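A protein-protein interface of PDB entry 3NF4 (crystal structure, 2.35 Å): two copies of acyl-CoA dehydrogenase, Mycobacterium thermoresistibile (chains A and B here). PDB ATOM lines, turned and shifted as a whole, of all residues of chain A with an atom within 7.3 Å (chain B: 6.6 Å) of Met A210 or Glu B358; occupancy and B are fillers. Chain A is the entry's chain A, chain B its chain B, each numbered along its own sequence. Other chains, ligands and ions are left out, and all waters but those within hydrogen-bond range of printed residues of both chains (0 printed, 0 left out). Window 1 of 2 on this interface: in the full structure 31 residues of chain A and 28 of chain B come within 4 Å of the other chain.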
ATOM      1  N   GLU A  46       3.473 -14.024 -20.811  1.00  0.00           N
ATOM      2  CA  GLU A  46       3.483 -13.109 -19.641  1.00  0.00           C
ATOM      3  C   GLU A  46       4.883 -12.950 -19.024  1.00  0.00           C
ATOM      4  O   GLU A  46       5.064 -12.977 -17.808  1.00  0.00           O
ATOM      5  CB  GLU A  46       2.379 -13.459 -18.604  1.00  0.00           C
ATOM      6  CG  GLU A  46       0.994 -13.663 -19.261  1.00  0.00           C
ATOM      7  CD  GLU A  46      -0.219 -13.686 -18.297  1.00  0.00           C
ATOM      8  OE1 GLU A  46      -0.118 -13.213 -17.141  1.00  0.00           O
ATOM      9  OE2 GLU A  46      -1.297 -14.178 -18.708  1.00  0.00           O
ATOM     10  N   GLU A 207       0.175  -8.815 -10.314  1.00  0.00           N
ATOM     11  CA  GLU A 207      -1.265  -8.963 -10.600  1.00  0.00           C
ATOM     12  C   GLU A 207      -1.521  -9.755 -11.877  1.00  0.00           C
ATOM     13  O   GLU A 207      -0.827  -9.563 -12.881  1.00  0.00           O
ATOM     14  CB  GLU A 207      -1.942  -7.591 -10.767  1.00  0.00           C
ATOM     15  CG  GLU A 207      -1.940  -6.697  -9.527  1.00  0.00           C
ATOM     16  CD  GLU A 207      -2.758  -7.253  -8.359  1.00  0.00           C
ATOM     17  OE1 GLU A 207      -3.840  -7.844  -8.583  1.00  0.00           O
ATOM     18  OE2 GLU A 207      -2.303  -7.083  -7.207  1.00  0.00           O
ATOM     19  N   GLU A 208      -2.524 -10.622 -11.824  1.00  0.00           N
ATOM     20  CA  GLU A 208      -3.037 -11.355 -12.986  1.00  0.00           C
ATOM     21  C   GLU A 208      -4.150 -10.538 -13.694  1.00  0.00           C
ATOM     22  O   GLU A 208      -5.290 -10.511 -13.229  1.00  0.00           O
ATOM     23  CB  GLU A 208      -3.640 -12.702 -12.531  1.00  0.00           C
ATOM     24  CG  GLU A 208      -2.669 -13.704 -11.904  1.00  0.00           C
ATOM     25  CD  GLU A 208      -3.391 -14.789 -11.091  1.00  0.00           C
ATOM     26  OE1 GLU A 208      -4.412 -14.466 -10.412  1.00  0.00           O
ATOM     27  OE2 GLU A 208      -2.929 -15.959 -11.111  1.00  0.00           O
ATOM     28  N   LYS A 209      -3.817  -9.921 -14.827  1.00  0.00           N
ATOM     29  CA  LYS A 209      -4.707  -8.964 -15.498  1.00  0.00           C
ATOM     30  C   LYS A 209      -5.362  -9.536 -16.746  1.00  0.00           C
ATOM     31  O   LYS A 209      -4.954 -10.581 -17.225  1.00  0.00           O
ATOM     32  CB  LYS A 209      -3.956  -7.668 -15.821  1.00  0.00           C
ATOM     33  CG  LYS A 209      -3.162  -7.083 -14.624  1.00  0.00           C
ATOM     34  CD  LYS A 209      -2.664  -5.666 -14.848  1.00  0.00           C
ATOM     35  CE  LYS A 209      -1.568  -5.564 -15.946  1.00  0.00           C
ATOM     36  NZ  LYS A 209      -0.269  -6.240 -15.593  1.00  0.00           N
ATOM     37  N   MET A 210      -6.404  -8.860 -17.239  1.00  0.00           N
ATOM     38  CA  MET A 210      -7.053  -9.194 -18.512  1.00  0.00           C
ATOM     39  C   MET A 210      -6.102  -9.038 -19.721  1.00  0.00           C
ATOM     40  O   MET A 210      -6.273  -9.745 -20.722  1.00  0.00           O
ATOM     41  CB  MET A 210      -8.306  -8.325 -18.703  1.00  0.00           C
ATOM     42  CG  MET A 210      -9.106  -8.573 -19.968  1.00  0.00           C
ATOM     43  SD  MET A 210     -10.620  -7.553 -20.165  1.00  0.00           S
ATOM     44  CE  MET A 210     -10.166  -6.076 -19.288  1.00  0.00           C
ATOM     45  N   GLY A 211      -5.131  -8.121 -19.633  1.00  0.00           N
ATOM     46  CA  GLY A 211      -4.154  -7.856 -20.727  1.00  0.00           C
ATOM     47  C   GLY A 211      -2.998  -6.958 -20.259  1.00  0.00           C
ATOM     48  O   GLY A 211      -2.918  -6.605 -19.063  1.00  0.00           O
ATOM     49  N   LEU A 212      -2.109  -6.594 -21.182  1.00  0.00           N
ATOM     50  CA  LEU A 212      -0.964  -5.704 -20.884  1.00  0.00           C
ATOM     51  C   LEU A 212       0.017  -6.391 -19.926  1.00  0.00           C
ATOM     52  O   LEU A 212       0.383  -5.848 -18.883  1.00  0.00           O
ATOM     53  CB  LEU A 212      -1.473  -4.387 -20.290  1.00  0.00           C
ATOM     54  CG  LEU A 212      -0.863  -3.018 -20.598  1.00  0.00           C
ATOM     55  CD1 LEU A 212      -1.259  -2.485 -22.008  1.00  0.00           C
ATOM     56  CD2 LEU A 212      -1.270  -1.990 -19.475  1.00  0.00           C
ATOM     57  N   HIS A 213       0.423  -7.604 -20.278  1.00  0.00           N
ATOM     58  CA  HIS A 213       1.047  -8.537 -19.327  1.00  0.00           C
ATOM     59  C   HIS A 213       2.548  -8.355 -19.100  1.00  0.00           C
ATOM     60  O   HIS A 213       3.031  -8.679 -18.005  1.00  0.00           O
ATOM     61  CB  HIS A 213       0.839  -9.987 -19.768  1.00  0.00           C
ATOM     62  CG  HIS A 213      -0.594 -10.385 -19.952  1.00  0.00           C
ATOM     63  ND1 HIS A 213      -1.487 -10.470 -18.903  1.00  0.00           N
ATOM     64  CD2 HIS A 213      -1.269 -10.786 -21.052  1.00  0.00           C
ATOM     65  CE1 HIS A 213      -2.662 -10.878 -19.354  1.00  0.00           C
ATOM     66  NE2 HIS A 213      -2.556 -11.080 -20.657  1.00  0.00           N
ATOM     67  N   GLU A 358      -7.893  -9.322 -31.018  1.00  0.00           N
ATOM     68  CA  GLU A 358      -8.500  -9.724 -29.737  1.00  0.00           C
ATOM     69  C   GLU A 358      -7.641  -9.255 -28.563  1.00  0.00           C
ATOM     70  O   GLU A 358      -8.177  -8.860 -27.521  1.00  0.00           O
ATOM     71  CB  GLU A 358      -8.795 -11.226 -29.671  1.00  0.00           C
ATOM     72  CG  GLU A 358      -7.537 -12.127 -29.581  1.00  0.00           C
ATOM     73  CD  GLU A 358      -6.972 -12.245 -28.148  1.00  0.00           C
ATOM     74  OE1 GLU A 358      -5.751 -12.542 -27.999  1.00  0.00           O
ATOM     75  OE2 GLU A 358      -7.759 -12.012 -27.191  1.00  0.00           O
ATOM     76  N   ARG A 359      -6.314  -9.254 -28.743  1.00  0.00           N
ATOM     77  CA  ARG A 359      -5.425  -8.666 -27.736  1.00  0.00           C
ATOM     78  C   ARG A 359      -5.616  -7.129 -27.605  1.00  0.00           C
ATOM     79  O   ARG A 359      -5.638  -6.589 -26.483  1.00  0.00           O
ATOM     80  CB  ARG A 359      -3.960  -9.021 -28.040  1.00  0.00           C
ATOM     81  CG  ARG A 359      -2.937  -8.304 -27.135  1.00  0.00           C
ATOM     82  CD  ARG A 359      -1.490  -8.939 -27.169  1.00  0.00           C
ATOM     83  NE  ARG A 359      -0.839  -8.891 -28.496  1.00  0.00           N
ATOM     84  CZ  ARG A 359      -0.153  -7.854 -28.986  1.00  0.00           C
ATOM     85  NH1 ARG A 359       0.008  -6.722 -28.301  1.00  0.00           N
ATOM     86  NH2 ARG A 359       0.397  -7.947 -30.190  1.00  0.00           N
ATOM     87  N   MET A 361      -8.227  -5.214 -28.169  1.00  0.00           N
ATOM     88  CA  MET A 361      -9.449  -5.031 -27.395  1.00  0.00           C
ATOM     89  C   MET A 361      -9.307  -5.210 -25.874  1.00  0.00           C
ATOM     90  O   MET A 361      -9.905  -4.471 -25.110  1.00  0.00           O
ATOM     91  CB  MET A 361     -10.568  -5.939 -27.931  1.00  0.00           C
ATOM     92  CG  MET A 361     -11.910  -5.606 -27.347  1.00  0.00           C
ATOM     93  SD  MET A 361     -13.268  -6.560 -28.069  1.00  0.00           S
ATOM     94  CE  MET A 361     -14.541  -6.306 -26.827  1.00  0.00           C
ATOM     95  N   ARG A 362      -8.542  -6.201 -25.444  1.00  0.00           N
ATOM     96  CA  ARG A 362      -8.259  -6.422 -24.022  1.00  0.00           C
ATOM     97  C   ARG A 362      -7.331  -5.316 -23.443  1.00  0.00           C
ATOM     98  O   ARG A 362      -7.512  -4.884 -22.303  1.00  0.00           O
ATOM     99  CB  ARG A 362      -7.657  -7.838 -23.779  1.00  0.00           C
ATOM    100  CG  ARG A 362      -8.611  -9.016 -24.128  1.00  0.00           C
ATOM    101  CD  ARG A 362      -8.001 -10.380 -23.746  1.00  0.00           C
ATOM    102  NE  ARG A 362      -7.017 -10.887 -24.718  1.00  0.00           N
ATOM    103  CZ  ARG A 362      -5.699 -10.980 -24.512  1.00  0.00           C
ATOM    104  NH1 ARG A 362      -5.148 -10.575 -23.371  1.00  0.00           N
ATOM    105  NH2 ARG A 362      -4.901 -11.461 -25.466  1.00  0.00           N
ATOM    106  N   GLU A 363      -6.392  -4.826 -24.234  1.00  0.00           N
ATOM    107  CA  GLU A 363      -5.507  -3.745 -23.800  1.00  0.00           C
ATOM    108  C   GLU A 363      -6.209  -2.394 -23.648  1.00  0.00           C
ATOM    109  O   GLU A 363      -5.831  -1.587 -22.791  1.00  0.00           O
ATOM    110  CB  GLU A 363      -4.300  -3.599 -24.754  1.00  0.00           C
ATOM    111  CG  GLU A 363      -3.265  -4.682 -24.537  1.00  0.00           C
ATOM    112  CD  GLU A 363      -2.227  -4.879 -25.675  1.00  0.00           C
ATOM    113  OE1 GLU A 363      -2.137  -4.082 -26.644  1.00  0.00           O
ATOM    114  OE2 GLU A 363      -1.474  -5.878 -25.573  1.00  0.00           O
ATOM    115  N   ALA A 364      -7.245  -2.142 -24.447  1.00  0.00           N
ATOM    116  CA  ALA A 364      -7.858  -0.807 -24.443  1.00  0.00           C
ATOM    117  C   ALA A 364      -8.692  -0.514 -23.183  1.00  0.00           C
ATOM    118  O   ALA A 364      -8.781   0.649 -22.762  1.00  0.00           O
ATOM    119  CB  ALA A 364      -8.705  -0.566 -25.750  1.00  0.00           C
ATOM    120  N   LYS A 365      -9.305  -1.559 -22.609  1.00  0.00           N
ATOM    121  CA  LYS A 365     -10.199  -1.405 -21.448  1.00  0.00           C
ATOM    122  C   LYS A 365      -9.545  -0.692 -20.251  1.00  0.00           C
ATOM    123  O   LYS A 365     -10.164   0.181 -19.664  1.00  0.00           O
ATOM    124  CB  LYS A 365     -10.815  -2.752 -21.012  1.00  0.00           C
ATOM    125  CG  LYS A 365     -11.789  -2.657 -19.852  1.00  0.00           C
ATOM    126  CD  LYS A 365     -13.052  -1.800 -20.197  1.00  0.00           C
ATOM    127  CE  LYS A 365     -13.196  -0.628 -19.221  1.00  0.00           C
ATOM    128  NZ  LYS A 365     -14.397   0.235 -19.469  1.00  0.00           N
ATOM    129  N   ILE A 366      -8.307  -1.050 -19.901  1.00  0.00           N
ATOM    130  CA  ILE A 366      -7.626  -0.469 -18.701  1.00  0.00           C
ATOM    131  C   ILE A 366      -7.272   1.026 -18.911  1.00  0.00           C
ATOM    132  O   ILE A 366      -7.178   1.810 -17.964  1.00  0.00           O
ATOM    133  CB  ILE A 366      -6.348  -1.293 -18.303  1.00  0.00           C
ATOM    134  CG1 ILE A 366      -5.719  -0.829 -16.951  1.00  0.00           C
ATOM    135  CG2 ILE A 366      -5.278  -1.186 -19.384  1.00  0.00           C
ATOM    136  CD1 ILE A 366      -6.691  -0.743 -15.726  1.00  0.00           C
ATOM    137  N   ILE A 369      -9.452   3.461 -17.451  1.00  0.00           N
ATOM    138  CA  ILE A 369      -9.427   3.343 -15.996  1.00  0.00           C
ATOM    139  C   ILE A 369      -8.226   4.029 -15.317  1.00  0.00           C
ATOM    140  O   ILE A 369      -8.424   4.811 -14.390  1.00  0.00           O
ATOM    141  CB  ILE A 369      -9.556   1.855 -15.525  1.00  0.00           C
ATOM    142  CG1 ILE A 369     -11.002   1.375 -15.696  1.00  0.00           C
ATOM    143  CG2 ILE A 369      -9.111   1.689 -14.076  1.00  0.00           C
ATOM    144  CD1 ILE A 369     -11.168  -0.121 -15.922  1.00  0.00           C
ATOM    145  N   THR B 339     -21.347  -5.077 -20.239  1.00  0.00           N
ATOM    146  CA  THR B 339     -20.161  -5.755 -19.706  1.00  0.00           C
ATOM    147  C   THR B 339     -18.956  -4.838 -19.726  1.00  0.00           C
ATOM    148  O   THR B 339     -18.136  -4.883 -18.798  1.00  0.00           O
ATOM    149  CB  THR B 339     -19.787  -7.018 -20.500  1.00  0.00           C
ATOM    150  OG1 THR B 339     -19.609  -6.685 -21.899  1.00  0.00           O
ATOM    151  CG2 THR B 339     -20.838  -8.093 -20.343  1.00  0.00           C
ATOM    152  N   VAL B 343     -17.000  -3.580 -15.877  1.00  0.00           N
ATOM    153  CA  VAL B 343     -15.551  -3.424 -15.582  1.00  0.00           C
ATOM    154  C   VAL B 343     -15.218  -1.979 -15.091  1.00  0.00           C
ATOM    155  O   VAL B 343     -14.543  -1.785 -14.066  1.00  0.00           O
ATOM    156  CB  VAL B 343     -14.624  -3.782 -16.825  1.00  0.00           C
ATOM    157  CG1 VAL B 343     -13.107  -3.568 -16.499  1.00  0.00           C
ATOM    158  CG2 VAL B 343     -14.854  -5.198 -17.321  1.00  0.00           C
ATOM    159  N   GLY B 350     -11.428  -4.590 -11.344  1.00  0.00           N
ATOM    160  CA  GLY B 350     -12.262  -5.139 -12.416  1.00  0.00           C
ATOM    161  C   GLY B 350     -11.436  -5.629 -13.592  1.00  0.00           C
ATOM    162  O   GLY B 350     -11.890  -6.488 -14.365  1.00  0.00           O
ATOM    163  N   TYR B 351     -10.216  -5.109 -13.704  1.00  0.00           N
ATOM    164  CA  TYR B 351      -9.281  -5.540 -14.748  1.00  0.00           C
ATOM    165  C   TYR B 351      -8.456  -6.785 -14.365  1.00  0.00           C
ATOM    166  O   TYR B 351      -7.626  -7.221 -15.155  1.00  0.00           O
ATOM    167  CB  TYR B 351      -8.363  -4.364 -15.144  1.00  0.00           C
ATOM    168  CG  TYR B 351      -7.621  -4.521 -16.459  1.00  0.00           C
ATOM    169  CD1 TYR B 351      -8.287  -4.439 -17.685  1.00  0.00           C
ATOM    170  CD2 TYR B 351      -6.244  -4.720 -16.478  1.00  0.00           C
ATOM    171  CE1 TYR B 351      -7.593  -4.574 -18.904  1.00  0.00           C
ATOM    172  CE2 TYR B 351      -5.530  -4.850 -17.687  1.00  0.00           C
ATOM    173  CZ  TYR B 351      -6.212  -4.764 -18.891  1.00  0.00           C
ATOM    174  OH  TYR B 351      -5.512  -4.891 -20.067  1.00  0.00           O
ATOM    175  N   THR B 352      -8.710  -7.367 -13.186  1.00  0.00           N
ATOM    176  CA  THR B 352      -7.982  -8.561 -12.702  1.00  0.00           C
ATOM    177  C   THR B 352      -8.876  -9.812 -12.738  1.00  0.00           C
ATOM    178  O   THR B 352     -10.090  -9.690 -12.831  1.00  0.00           O
ATOM    179  CB  THR B 352      -7.412  -8.383 -11.231  1.00  0.00           C
ATOM    180  OG1 THR B 352      -8.499  -8.297 -10.293  1.00  0.00           O
ATOM    181  CG2 THR B 352      -6.577  -7.124 -11.096  1.00  0.00           C
ATOM    182  N   ARG B 353      -8.287 -11.002 -12.636  1.00  0.00           N
ATOM    183  CA  ARG B 353      -9.066 -12.253 -12.647  1.00  0.00           C
ATOM    184  C   ARG B 353      -9.489 -12.689 -11.241  1.00  0.00           C
ATOM    185  O   ARG B 353      -9.842 -13.839 -11.030  1.00  0.00           O
ATOM    186  CB  ARG B 353      -8.326 -13.419 -13.344  1.00  0.00           C
ATOM    187  CG  ARG B 353      -7.338 -13.041 -14.427  1.00  0.00           C
ATOM    188  CD  ARG B 353      -6.677 -14.273 -15.067  1.00  0.00           C
ATOM    189  NE  ARG B 353      -5.839 -13.877 -16.205  1.00  0.00           N
ATOM    190  CZ  ARG B 353      -4.528 -14.126 -16.322  1.00  0.00           C
ATOM    191  NH1 ARG B 353      -3.875 -14.818 -15.379  1.00  0.00           N
ATOM    192  NH2 ARG B 353      -3.869 -13.710 -17.413  1.00  0.00           N
ATOM    193  N   ASP B 354      -9.463 -11.768 -10.283  1.00  0.00           N
ATOM    194  CA  ASP B 354     -10.049 -12.003  -8.962  1.00  0.00           C
ATOM    195  C   ASP B 354     -11.565 -11.820  -9.007  1.00  0.00           C
ATOM    196  O   ASP B 354     -12.273 -12.155  -8.046  1.00  0.00           O
ATOM    197  CB  ASP B 354      -9.487 -11.016  -7.944  1.00  0.00           C
ATOM    198  CG  ASP B 354      -8.024 -11.307  -7.560  1.00  0.00           C
ATOM    199  OD1 ASP B 354      -7.370 -12.225  -8.144  1.00  0.00           O
ATOM    200  OD2 ASP B 354      -7.539 -10.577  -6.652  1.00  0.00           O
ATOM    201  N   TYR B 355     -12.050 -11.254 -10.112  1.00  0.00           N
ATOM    202  CA  TYR B 355     -13.475 -11.056 -10.319  1.00  0.00           C
ATOM    203  C   TYR B 355     -13.902 -11.614 -11.677  1.00  0.00           C
ATOM    204  O   TYR B 355     -13.070 -11.892 -12.523  1.00  0.00           O
ATOM    205  CB  TYR B 355     -13.800  -9.577 -10.195  1.00  0.00           C
ATOM    206  CG  TYR B 355     -13.679  -9.077  -8.791  1.00  0.00           C
ATOM    207  CD1 TYR B 355     -12.575  -8.345  -8.393  1.00  0.00           C
ATOM    208  CD2 TYR B 355     -14.677  -9.349  -7.845  1.00  0.00           C
ATOM    209  CE1 TYR B 355     -12.462  -7.880  -7.095  1.00  0.00           C
ATOM    210  CE2 TYR B 355     -14.575  -8.895  -6.544  1.00  0.00           C
ATOM    211  CZ  TYR B 355     -13.465  -8.166  -6.174  1.00  0.00           C
ATOM    212  OH  TYR B 355     -13.361  -7.708  -4.887  1.00  0.00           O
ATOM    213  N   ARG B 356     -15.200 -11.792 -11.867  1.00  0.00           N
ATOM    214  CA  ARG B 356     -15.742 -12.360 -13.091  1.00  0.00           C
ATOM    215  C   ARG B 356     -16.020 -11.353 -14.221  1.00  0.00           C
ATOM    216  O   ARG B 356     -16.177 -11.761 -15.362  1.00  0.00           O
ATOM    217  CB  ARG B 356     -17.036 -13.104 -12.776  1.00  0.00           C
ATOM    218  CG  ARG B 356     -16.886 -14.485 -12.155  1.00  0.00           C
ATOM    219  CD  ARG B 356     -18.279 -15.033 -11.754  1.00  0.00           C
ATOM    220  NE  ARG B 356     -18.160 -16.382 -11.174  1.00  0.00           N
ATOM    221  CZ  ARG B 356     -19.171 -17.103 -10.678  1.00  0.00           C
ATOM    222  NH1 ARG B 356     -20.429 -16.643 -10.685  1.00  0.00           N
ATOM    223  NH2 ARG B 356     -18.918 -18.304 -10.170  1.00  0.00           N
ATOM    224  N   VAL B 357     -16.078 -10.054 -13.930  1.00  0.00           N
ATOM    225  CA  VAL B 357     -16.466  -9.109 -14.977  1.00  0.00           C
ATOM    226  C   VAL B 357     -15.547  -9.037 -16.229  1.00  0.00           C
ATOM    227  O   VAL B 357     -16.031  -8.774 -17.324  1.00  0.00           O
ATOM    228  CB  VAL B 357     -16.899  -7.699 -14.437  1.00  0.00           C
ATOM    229  CG1 VAL B 357     -18.121  -7.834 -13.548  1.00  0.00           C
ATOM    230  CG2 VAL B 357     -15.777  -7.003 -13.707  1.00  0.00           C
ATOM    231  N   GLU B 358     -14.254  -9.290 -16.076  1.00  0.00           N
ATOM    232  CA  GLU B 358     -13.339  -9.332 -17.226  1.00  0.00           C
ATOM    233  C   GLU B 358     -13.686 -10.523 -18.174  1.00  0.00           C
ATOM    234  O   GLU B 358     -13.716 -10.359 -19.407  1.00  0.00           O
ATOM    235  CB  GLU B 358     -11.859  -9.345 -16.755  1.00  0.00           C
ATOM    236  CG  GLU B 358     -11.375 -10.642 -16.046  1.00  0.00           C
ATOM    237  CD  GLU B 358     -10.851 -11.663 -17.059  1.00  0.00           C
ATOM    238  OE1 GLU B 358     -10.800 -12.879 -16.763  1.00  0.00           O
ATOM    239  OE2 GLU B 358     -10.509 -11.226 -18.182  1.00  0.00           O
ATOM    240  N   ARG B 359     -13.979 -11.693 -17.604  1.00  0.00           N
ATOM    241  CA  ARG B 359     -14.486 -12.833 -18.382  1.00  0.00           C
ATOM    242  C   ARG B 359     -15.821 -12.512 -19.119  1.00  0.00           C
ATOM    243  O   ARG B 359     -15.984 -12.840 -20.319  1.00  0.00           O
ATOM    244  CB  ARG B 359     -14.615 -14.106 -17.493  1.00  0.00           C
ATOM    245  CG  ARG B 359     -15.239 -15.310 -18.236  1.00  0.00           C
ATOM    246  CD  ARG B 359     -15.119 -16.680 -17.511  1.00  0.00           C
ATOM    247  NE  ARG B 359     -15.797 -16.723 -16.218  1.00  0.00           N
ATOM    248  CZ  ARG B 359     -17.086 -16.997 -16.018  1.00  0.00           C
ATOM    249  NH1 ARG B 359     -17.901 -17.277 -17.036  1.00  0.00           N
ATOM    250  NH2 ARG B 359     -17.569 -16.969 -14.773  1.00  0.00           N
ATOM    251  N   TYR B 360     -16.767 -11.852 -18.445  1.00  0.00           N
ATOM    252  CA  TYR B 360     -18.064 -11.555 -19.118  1.00  0.00           C
ATOM    253  C   TYR B 360     -17.906 -10.629 -20.340  1.00  0.00           C
ATOM    254  O   TYR B 360     -18.616 -10.775 -21.351  1.00  0.00           O
ATOM    255  CB  TYR B 360     -19.080 -10.950 -18.144  1.00  0.00           C
ATOM    256  CG  TYR B 360     -19.580 -11.854 -17.035  1.00  0.00           C
ATOM    257  CD1 TYR B 360     -19.530 -13.262 -17.151  1.00  0.00           C
ATOM    258  CD2 TYR B 360     -20.133 -11.300 -15.860  1.00  0.00           C
ATOM    259  CE1 TYR B 360     -19.994 -14.088 -16.123  1.00  0.00           C
ATOM    260  CE2 TYR B 360     -20.603 -12.144 -14.807  1.00  0.00           C
ATOM    261  CZ  TYR B 360     -20.533 -13.525 -14.956  1.00  0.00           C
ATOM    262  OH  TYR B 360     -21.027 -14.360 -13.941  1.00  0.00           O
ATOM    263  N   MET B 361     -16.993  -9.666 -20.244  1.00  0.00           N
ATOM    264  CA  MET B 361     -16.687  -8.776 -21.375  1.00  0.00           C
ATOM    265  C   MET B 361     -16.095  -9.552 -22.557  1.00  0.00           C
ATOM    266  O   MET B 361     -16.462  -9.304 -23.725  1.00  0.00           O
ATOM    267  CB  MET B 361     -15.761  -7.626 -20.928  1.00  0.00           C
ATOM    268  CG  MET B 361     -15.532  -6.522 -21.927  1.00  0.00           C
ATOM    269  SD  MET B 361     -14.409  -5.184 -21.366  1.00  0.00           S
ATOM    270  CE  MET B 361     -14.268  -4.246 -22.895  1.00  0.00           C
ATOM    271  N   ARG B 362     -15.190 -10.492 -22.277  1.00  0.00           N
ATOM    272  CA  ARG B 362     -14.663 -11.350 -23.358  1.00  0.00           C
ATOM    273  C   ARG B 362     -15.771 -12.222 -24.029  1.00  0.00           C
ATOM    274  O   ARG B 362     -15.797 -12.351 -25.252  1.00  0.00           O
ATOM    275  CB  ARG B 362     -13.453 -12.200 -22.895  1.00  0.00           C
ATOM    276  CG  ARG B 362     -12.239 -11.392 -22.372  1.00  0.00           C
ATOM    277  CD  ARG B 362     -11.026 -12.297 -21.981  1.00  0.00           C
ATOM    278  NE  ARG B 362     -11.102 -12.861 -20.619  1.00  0.00           N
ATOM    279  CZ  ARG B 362     -11.343 -14.141 -20.333  1.00  0.00           C
ATOM    280  NH1 ARG B 362     -11.571 -15.010 -21.321  1.00  0.00           N
ATOM    281  NH2 ARG B 362     -11.413 -14.554 -19.052  1.00  0.00           N
ATOM    282  N   GLU B 363     -16.698 -12.773 -23.243  1.00  0.00           N
ATOM    283  CA  GLU B 363     -17.797 -13.592 -23.788  1.00  0.00           C
ATOM    284  C   GLU B 363     -18.785 -12.826 -24.669  1.00  0.00           C
ATOM    285  O   GLU B 363     -19.385 -13.425 -25.571  1.00  0.00           O
ATOM    286  CB  GLU B 363     -18.559 -14.362 -22.657  1.00  0.00           C
ATOM    287  CG  GLU B 363     -17.626 -15.335 -21.899  1.00  0.00           C
ATOM    288  CD  GLU B 363     -18.183 -15.988 -20.623  1.00  0.00           C
ATOM    289  OE1 GLU B 363     -19.259 -15.591 -20.094  1.00  0.00           O
ATOM    290  OE2 GLU B 363     -17.507 -16.936 -20.155  1.00  0.00           O
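Printed residues of chain A that touch a printed residue of chain B: Glu A46, Glu A207, Glu A208, Lys A209, Met A210, Gly A211, Leu A212, His A213, Arg A362, Glu A363, Lys A365, Ile A366 and Ile A369. Among the printed residues, 18 pairs touch across the chains.
OE2 of Glu A46 lies within salt-bridge range of NH2 of Arg B353, at 2.9 Å. The backbone carbonyl oxygen (O) of Glu A208 sits at hydrogen-bond distance from the backbone NH (N) of Arg B353 (3.1 Å). O of Lys A209 lies within hydrogen-bond range of NH2 of Arg B353. The backbone NH of Met A210 sits at hydrogen-bond distance from the backbone carbonyl oxygen of Tyr B351 (2.9 Å). OH of Tyr B351 sits close to O of Gly A211, at 3.3 Å. The side-chain hydroxyl (OH) of Tyr B351 lies within hydrogen-bond range of the backbone carbonyl oxygen (O) of Arg A362, 3.0 Å away.
Arg B362 touches its own counterpart, Arg A362. 5 positions are printed for both chains.
Among the printed residues, merely in contact across the chains: Glu A208 with Thr B352, Lys A209 with Tyr B351, Met A210 with Glu B358, Ile A366 with Tyr B351, His A213 with Arg B353, Lys A365 with Val B343, Glu A207 with Thr B352, Lys A365 with Met B361, Glu A363 with Tyr B351, Leu A212 with Tyr B351, Arg A362 with Arg B362 and Ile A369 with Val B343.
Printed residues of chain B within 4 Å of Glu A208: Thr B352 (3.4 Å) and Arg B353 (3.1 Å). Of the printed residues of chain B, Met A210 touches Tyr B351 (2.9 Å) and Glu B358 (3.5 Å). Of the printed residues of chain B, Glu A363 touches Tyr B351. Printed residues of chain A within 4 Å of Arg B353: Glu A46 (2.9 Å), Glu A208 (3.1 Å), Lys A209 (3.3 Å) and His A213 (3.6 Å). Glu B358 touches one residue of chain A. The nearest residue of chain A that does not touch Glu B358 is Lys A209 (5.6 Å).
The backbone carbonyl oxygen (O) of Leu A212 lies within hydrogen-bond range of the side-chain amino group (NZ) of Lys A209 (3.4 Å). The backbone carbonyl oxygen (O) of Met A210 sits at hydrogen-bond distance from the guanidinium group (NH1) of Arg A362. OE2 of Glu A358 is in salt-bridge range of NE of Arg A362. The guanidinium group (NH1) of Arg A359 is in salt-bridge range of the side-chain carboxylate (OE2) of Glu A363, at 3.2 Å. The side-chain carboxylate (OE1) of Glu B358 is in salt-bridge range of the guanidinium group (NH2) of Arg B362 (2.9 Å).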
